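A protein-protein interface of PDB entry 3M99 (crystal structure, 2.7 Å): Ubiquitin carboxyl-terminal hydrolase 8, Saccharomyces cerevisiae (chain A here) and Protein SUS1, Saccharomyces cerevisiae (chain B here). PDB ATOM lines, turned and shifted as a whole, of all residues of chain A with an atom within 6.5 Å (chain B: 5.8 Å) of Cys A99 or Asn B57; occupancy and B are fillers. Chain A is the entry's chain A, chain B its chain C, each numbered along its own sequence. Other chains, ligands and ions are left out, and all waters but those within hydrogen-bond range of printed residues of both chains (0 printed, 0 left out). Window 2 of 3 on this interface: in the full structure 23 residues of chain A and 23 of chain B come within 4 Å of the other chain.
Among the printed residues, pairs that only touch across the chains: Tyr A102 with Phe B58, Asp A101 with Asn B57, Glu A100 with Asn B57 and Cys A99 with Asn B57.
Pro A5 touches none of the printed residues of chain B.
Of chain B, only Asn B57 (3.95 Å) comes within 4 Å of Cys A99.
Of the printed residues of chain B, Glu A100 touches Asn B57 and Thr B59.
Of the printed residues of chain B, Tyr A102 touches Phe B58 (3.1 Å).
Ile A103 touches none of the printed residues of chain B.
Asn B57 touches just these residues of chain A: Cys A99, Glu A100 and Asp A101.
OG1 of Thr B59 lies within hydrogen-bond range of O of Glu A100 (2.5 Å).
The side-chain carboxylate of Asp A101 is in hydrogen-bond range of the backbone NH of Phe B58 (2.7 Å).
O of Thr B56 sits close to OD2 of Asp A101, 2.9 Å away.
SG of Cys A4 forms a disulfide with SG of Cys A99, at 2.1 Å.
The backbone carbonyl oxygen (O) of Asp A101 lies within hydrogen-bond range of the backbone NH (N) of Cys A96 (3.1 Å).
OG of Ser B55 lies within hydrogen-bond range of N of Asn B57 (3.2 Å).
OD1 of Asn B57 lies within hydrogen-bond range of N of Thr B59 (3.2 Å).
The side-chain amide oxygen of Asn B57 lies within hydrogen-bond range of the backbone NH of Gln B60 (2.8 Å).
SG of Cys A4 forms a disulfide with SG of Cys A96.
Of the 8 printed residues of chain B, 4 touch a printed residue of chain A.
Printed residues of chain B that touch a printed residue of chain A: Thr B56, Asn B57, Phe B58 and Thr B59.
Among the printed residues, 7 pairs touch across the chains.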
ATOM      1  N   ILE A   3      -6.588  10.879   4.715  1.00  0.00           N
ATOM      2  CA  ILE A   3      -7.066  10.569   3.379  1.00  0.00           C
ATOM      3  C   ILE A   3      -7.687   9.171   3.251  1.00  0.00           C
ATOM      4  O   ILE A   3      -8.906   9.039   3.144  1.00  0.00           O
ATOM      5  CB  ILE A   3      -5.966  10.839   2.308  1.00  0.00           C
ATOM      6  CG1 ILE A   3      -4.577  10.431   2.823  1.00  0.00           C
ATOM      7  CG2 ILE A   3      -5.957  12.325   1.921  1.00  0.00           C
ATOM      8  CD1 ILE A   3      -4.165   9.001   2.493  1.00  0.00           C
ATOM      9  N   CYS A   4      -6.858   8.136   3.294  1.00  0.00           N
ATOM     10  CA  CYS A   4      -7.308   6.797   2.933  1.00  0.00           C
ATOM     11  C   CYS A   4      -8.084   6.896   1.621  1.00  0.00           C
ATOM     12  O   CYS A   4      -9.316   6.895   1.622  1.00  0.00           O
ATOM     13  CB  CYS A   4      -8.176   6.167   4.036  1.00  0.00           C
ATOM     14  SG  CYS A   4      -8.173   4.327   4.044  1.00  0.00           S
ATOM     15  N   PRO A   5      -7.361   7.006   0.493  1.00  0.00           N
ATOM     16  CA  PRO A   5      -7.997   7.173  -0.817  1.00  0.00           C
ATOM     17  C   PRO A   5      -8.886   5.985  -1.105  1.00  0.00           C
ATOM     18  O   PRO A   5      -9.761   6.066  -1.958  1.00  0.00           O
ATOM     19  CB  PRO A   5      -6.805   7.183  -1.782  1.00  0.00           C
ATOM     20  CG  PRO A   5      -5.701   6.501  -1.011  1.00  0.00           C
ATOM     21  CD  PRO A   5      -5.895   6.997   0.377  1.00  0.00           C
ATOM     22  N   HIS A   6      -8.661   4.896  -0.381  1.00  0.00           N
ATOM     23  CA  HIS A   6      -9.454   3.688  -0.543  1.00  0.00           C
ATOM     24  C   HIS A   6     -10.957   3.950  -0.488  1.00  0.00           C
ATOM     25  O   HIS A   6     -11.660   3.712  -1.470  1.00  0.00           O
ATOM     26  CB  HIS A   6      -9.053   2.666   0.509  1.00  0.00           C
ATOM     27  CG  HIS A   6      -7.576   2.474   0.617  1.00  0.00           C
ATOM     28  ND1 HIS A   6      -6.772   3.296   1.378  1.00  0.00           N
ATOM     29  CD2 HIS A   6      -6.752   1.559   0.052  1.00  0.00           C
ATOM     30  CE1 HIS A   6      -5.519   2.889   1.283  1.00  0.00           C
ATOM     31  NE2 HIS A   6      -5.480   1.838   0.487  1.00  0.00           N
ATOM     32  N   ILE A   7     -11.456   4.436   0.647  1.00  0.00           N
ATOM     33  CA  ILE A   7     -12.884   4.712   0.756  1.00  0.00           C
ATOM     34  C   ILE A   7     -13.263   5.800  -0.237  1.00  0.00           C
ATOM     35  O   ILE A   7     -14.403   5.868  -0.693  1.00  0.00           O
ATOM     36  CB  ILE A   7     -13.307   5.144   2.182  1.00  0.00           C
ATOM     37  CG1 ILE A   7     -12.195   4.859   3.187  1.00  0.00           C
ATOM     38  CG2 ILE A   7     -14.628   4.481   2.589  1.00  0.00           C
ATOM     39  CD1 ILE A   7     -11.302   6.053   3.447  1.00  0.00           C
ATOM     40  N   PHE A  95     -12.561   1.014  10.427  1.00  0.00           N
ATOM     41  CA  PHE A  95     -11.116   0.904  10.299  1.00  0.00           C
ATOM     42  C   PHE A  95     -10.693   0.523   8.878  1.00  0.00           C
ATOM     43  O   PHE A  95     -11.211  -0.425   8.299  1.00  0.00           O
ATOM     44  CB  PHE A  95     -10.565  -0.104  11.307  1.00  0.00           C
ATOM     45  CG  PHE A  95      -9.080  -0.022  11.491  1.00  0.00           C
ATOM     46  CD1 PHE A  95      -8.526   0.967  12.286  1.00  0.00           C
ATOM     47  CD2 PHE A  95      -8.233  -0.929  10.867  1.00  0.00           C
ATOM     48  CE1 PHE A  95      -7.158   1.053  12.464  1.00  0.00           C
ATOM     49  CE2 PHE A  95      -6.854  -0.849  11.037  1.00  0.00           C
ATOM     50  CZ  PHE A  95      -6.317   0.144  11.837  1.00  0.00           C
ATOM     51  N   CYS A  96      -9.754   1.291   8.334  1.00  0.00           N
ATOM     52  CA  CYS A  96      -9.139   1.023   7.036  1.00  0.00           C
ATOM     53  C   CYS A  96      -7.876   0.197   7.289  1.00  0.00           C
ATOM     54  O   CYS A  96      -6.929   0.685   7.901  1.00  0.00           O
ATOM     55  CB  CYS A  96      -8.779   2.359   6.378  1.00  0.00           C
ATOM     56  SG  CYS A  96      -8.508   2.370   4.584  1.00  0.00           S
ATOM     57  N   PHE A  97      -7.865  -1.058   6.851  1.00  0.00           N
ATOM     58  CA  PHE A  97      -6.744  -1.945   7.163  1.00  0.00           C
ATOM     59  C   PHE A  97      -5.543  -1.818   6.221  1.00  0.00           C
ATOM     60  O   PHE A  97      -4.527  -2.483   6.427  1.00  0.00           O
ATOM     61  CB  PHE A  97      -7.203  -3.397   7.232  1.00  0.00           C
ATOM     62  CG  PHE A  97      -7.753  -3.794   8.565  1.00  0.00           C
ATOM     63  CD1 PHE A  97      -9.103  -3.655   8.841  1.00  0.00           C
ATOM     64  CD2 PHE A  97      -6.923  -4.312   9.546  1.00  0.00           C
ATOM     65  CE1 PHE A  97      -9.615  -4.023  10.070  1.00  0.00           C
ATOM     66  CE2 PHE A  97      -7.430  -4.684  10.778  1.00  0.00           C
ATOM     67  CZ  PHE A  97      -8.777  -4.540  11.037  1.00  0.00           C
ATOM     68  N   LYS A  98      -5.672  -0.985   5.189  1.00  0.00           N
ATOM     69  CA  LYS A  98      -4.536  -0.598   4.352  1.00  0.00           C
ATOM     70  C   LYS A  98      -3.867   0.663   4.914  1.00  0.00           C
ATOM     71  O   LYS A  98      -2.661   0.669   5.150  1.00  0.00           O
ATOM     72  CB  LYS A  98      -4.951  -0.384   2.887  1.00  0.00           C
ATOM     73  CG  LYS A  98      -5.023  -1.661   2.028  1.00  0.00           C
ATOM     74  CD  LYS A  98      -5.383  -1.331   0.572  1.00  0.00           C
ATOM     75  CE  LYS A  98      -5.335  -2.553  -0.350  1.00  0.00           C
ATOM     76  NZ  LYS A  98      -5.756  -2.217  -1.748  1.00  0.00           N
ATOM     77  N   CYS A  99      -4.652   1.723   5.128  1.00  0.00           N
ATOM     78  CA  CYS A  99      -4.162   2.935   5.784  1.00  0.00           C
ATOM     79  C   CYS A  99      -3.593   2.559   7.139  1.00  0.00           C
ATOM     80  O   CYS A  99      -2.603   3.127   7.600  1.00  0.00           O
ATOM     81  CB  CYS A  99      -5.287   3.952   6.002  1.00  0.00           C
ATOM     82  SG  CYS A  99      -6.185   4.507   4.536  1.00  0.00           S
ATOM     83  N   GLU A 100      -4.250   1.607   7.784  1.00  0.00           N
ATOM     84  CA  GLU A 100      -3.846   1.159   9.105  1.00  0.00           C
ATOM     85  C   GLU A 100      -4.234   2.188  10.176  1.00  0.00           C
ATOM     86  O   GLU A 100      -3.528   2.364  11.170  1.00  0.00           O
ATOM     87  CB  GLU A 100      -2.342   0.894   9.119  1.00  0.00           C
ATOM     88  CG  GLU A 100      -1.928  -0.314   9.931  1.00  0.00           C
ATOM     89  CD  GLU A 100      -0.438  -0.598   9.836  1.00  0.00           C
ATOM     90  OE1 GLU A 100      -0.014  -1.680  10.301  1.00  0.00           O
ATOM     91  OE2 GLU A 100       0.309   0.257   9.302  1.00  0.00           O
ATOM     92  N   ASP A 101      -5.358   2.868   9.959  1.00  0.00           N
ATOM     93  CA  ASP A 101      -5.851   3.886  10.886  1.00  0.00           C
ATOM     94  C   ASP A 101      -7.382   3.939  10.836  1.00  0.00           C
ATOM     95  O   ASP A 101      -8.003   3.280  10.002  1.00  0.00           O
ATOM     96  CB  ASP A 101      -5.261   5.258  10.539  1.00  0.00           C
ATOM     97  CG  ASP A 101      -5.385   6.261  11.684  1.00  0.00           C
ATOM     98  OD1 ASP A 101      -5.843   5.874  12.784  1.00  0.00           O
ATOM     99  OD2 ASP A 101      -5.018   7.440  11.483  1.00  0.00           O
ATOM    100  N   TYR A 102      -7.998   4.711  11.722  1.00  0.00           N
ATOM    101  CA  TYR A 102      -9.451   4.848  11.677  1.00  0.00           C
ATOM    102  C   TYR A 102      -9.871   5.863  10.611  1.00  0.00           C
ATOM    103  O   TYR A 102      -9.038   6.603  10.095  1.00  0.00           O
ATOM    104  CB  TYR A 102     -10.026   5.186  13.065  1.00  0.00           C
ATOM    105  CG  TYR A 102     -10.131   3.974  13.971  1.00  0.00           C
ATOM    106  CD1 TYR A 102     -11.237   3.131  13.912  1.00  0.00           C
ATOM    107  CD2 TYR A 102      -9.119   3.658  14.868  1.00  0.00           C
ATOM    108  CE1 TYR A 102     -11.340   2.015  14.723  1.00  0.00           C
ATOM    109  CE2 TYR A 102      -9.215   2.540  15.686  1.00  0.00           C
ATOM    110  CZ  TYR A 102     -10.331   1.722  15.608  1.00  0.00           C
ATOM    111  OH  TYR A 102     -10.449   0.607  16.413  1.00  0.00           O
ATOM    112  N   ILE A 103     -11.153   5.875  10.259  1.00  0.00           N
ATOM    113  CA  ILE A 103     -11.677   6.863   9.321  1.00  0.00           C
ATOM    114  C   ILE A 103     -12.640   7.823  10.046  1.00  0.00           C
ATOM    115  O   ILE A 103     -13.861   7.613  10.090  1.00  0.00           O
ATOM    116  CB  ILE A 103     -12.333   6.189   8.090  1.00  0.00           C
ATOM    117  CG1 ILE A 103     -11.353   5.212   7.442  1.00  0.00           C
ATOM    118  CG2 ILE A 103     -12.765   7.218   7.068  1.00  0.00           C
ATOM    119  CD1 ILE A 103     -11.990   4.283   6.435  1.00  0.00           C
ATOM    120  N   SER B  55       1.075  12.983  15.442  1.00  0.00           N
ATOM    121  CA  SER B  55       0.455  11.943  14.617  1.00  0.00           C
ATOM    122  C   SER B  55      -0.909  11.520  15.178  1.00  0.00           C
ATOM    123  O   SER B  55      -1.113  11.524  16.396  1.00  0.00           O
ATOM    124  CB  SER B  55       1.377  10.720  14.527  1.00  0.00           C
ATOM    125  OG  SER B  55       0.701   9.586  14.005  1.00  0.00           O
ATOM    126  N   THR B  56      -1.835  11.152  14.294  1.00  0.00           N
ATOM    127  CA  THR B  56      -3.145  10.649  14.719  1.00  0.00           C
ATOM    128  C   THR B  56      -3.412   9.240  14.189  1.00  0.00           C
ATOM    129  O   THR B  56      -4.565   8.827  14.036  1.00  0.00           O
ATOM    130  CB  THR B  56      -4.295  11.579  14.282  1.00  0.00           C
ATOM    131  OG1 THR B  56      -4.178  11.865  12.884  1.00  0.00           O
ATOM    132  CG2 THR B  56      -4.263  12.881  15.068  1.00  0.00           C
ATOM    133  N   ASN B  57      -2.337   8.509  13.912  1.00  0.00           N
ATOM    134  CA  ASN B  57      -2.436   7.155  13.385  1.00  0.00           C
ATOM    135  C   ASN B  57      -2.660   6.150  14.510  1.00  0.00           C
ATOM    136  O   ASN B  57      -1.874   6.070  15.451  1.00  0.00           O
ATOM    137  CB  ASN B  57      -1.176   6.813  12.579  1.00  0.00           C
ATOM    138  CG  ASN B  57      -1.198   5.403  12.012  1.00  0.00           C
ATOM    139  OD1 ASN B  57      -0.913   4.430  12.714  1.00  0.00           O
ATOM    140  ND2 ASN B  57      -1.516   5.288  10.728  1.00  0.00           N
ATOM    141  N   PHE B  58      -3.739   5.385  14.413  1.00  0.00           N
ATOM    142  CA  PHE B  58      -4.115   4.478  15.487  1.00  0.00           C
ATOM    143  C   PHE B  58      -3.024   3.476  15.871  1.00  0.00           C
ATOM    144  O   PHE B  58      -2.680   3.360  17.050  1.00  0.00           O
ATOM    145  CB  PHE B  58      -5.408   3.737  15.154  1.00  0.00           C
ATOM    146  CG  PHE B  58      -5.807   2.748  16.199  1.00  0.00           C
ATOM    147  CD1 PHE B  58      -6.583   3.137  17.273  1.00  0.00           C
ATOM    148  CD2 PHE B  58      -5.387   1.434  16.121  1.00  0.00           C
ATOM    149  CE1 PHE B  58      -6.943   2.231  18.240  1.00  0.00           C
ATOM    150  CE2 PHE B  58      -5.744   0.525  17.086  1.00  0.00           C
ATOM    151  CZ  PHE B  58      -6.524   0.924  18.147  1.00  0.00           C
ATOM    152  N   THR B  59      -2.500   2.750  14.883  1.00  0.00           N
ATOM    153  CA  THR B  59      -1.495   1.713  15.119  1.00  0.00           C
ATOM    154  C   THR B  59      -0.260   2.334  15.737  1.00  0.00           C
ATOM    155  O   THR B  59       0.367   1.768  16.637  1.00  0.00           O
ATOM    156  CB  THR B  59      -1.056   1.036  13.804  1.00  0.00           C
ATOM    157  OG1 THR B  59      -2.087   1.162  12.815  1.00  0.00           O
ATOM    158  CG2 THR B  59      -0.736  -0.433  14.041  1.00  0.00           C
ATOM    159  N   GLN B  60       0.067   3.516  15.227  1.00  0.00           N
ATOM    160  CA  GLN B  60       1.259   4.268  15.592  1.00  0.00           C
ATOM    161  C   GLN B  60       1.192   4.732  17.049  1.00  0.00           C
ATOM    162  O   GLN B  60       2.136   4.554  17.821  1.00  0.00           O
ATOM    163  CB  GLN B  60       1.372   5.470  14.645  1.00  0.00           C
ATOM    164  CG  GLN B  60       2.780   5.897  14.272  1.00  0.00           C
ATOM    165  CD  GLN B  60       3.371   6.891  15.255  1.00  0.00           C
ATOM    166  OE1 GLN B  60       3.930   6.506  16.282  1.00  0.00           O
ATOM    167  NE2 GLN B  60       3.254   8.178  14.938  1.00  0.00           N
ATOM    168  N   ILE B  61       0.063   5.326  17.419  1.00  0.00           N
ATOM    169  CA  ILE B  61      -0.140   5.806  18.779  1.00  0.00           C
ATOM    170  C   ILE B  61      -0.389   4.660  19.770  1.00  0.00           C
ATOM    171  O   ILE B  61       0.011   4.739  20.933  1.00  0.00           O
ATOM    172  CB  ILE B  61      -1.293   6.840  18.845  1.00  0.00           C
ATOM    173  CG1 ILE B  61      -1.022   8.010  17.886  1.00  0.00           C
ATOM    174  CG2 ILE B  61      -1.511   7.327  20.277  1.00  0.00           C
ATOM    175  CD1 ILE B  61       0.244   8.781  18.184  1.00  0.00           C
ATOM    176  N   LEU B  62      -1.035   3.595  19.304  1.00  0.00           N
ATOM    177  CA  LEU B  62      -1.352   2.459  20.165  1.00  0.00           C
ATOM    178  C   LEU B  62      -0.121   1.709  20.665  1.00  0.00           C
ATOM    179  O   LEU B  62      -0.121   1.191  21.781  1.00  0.00           O
ATOM    180  CB  LEU B  62      -2.284   1.477  19.455  1.00  0.00           C
ATOM    181  CG  LEU B  62      -2.425   0.109  20.135  1.00  0.00           C
ATOM    182  CD1 LEU B  62      -3.123   0.220  21.486  1.00  0.00           C
ATOM    183  CD2 LEU B  62      -3.168  -0.858  19.242  1.00  0.00           C
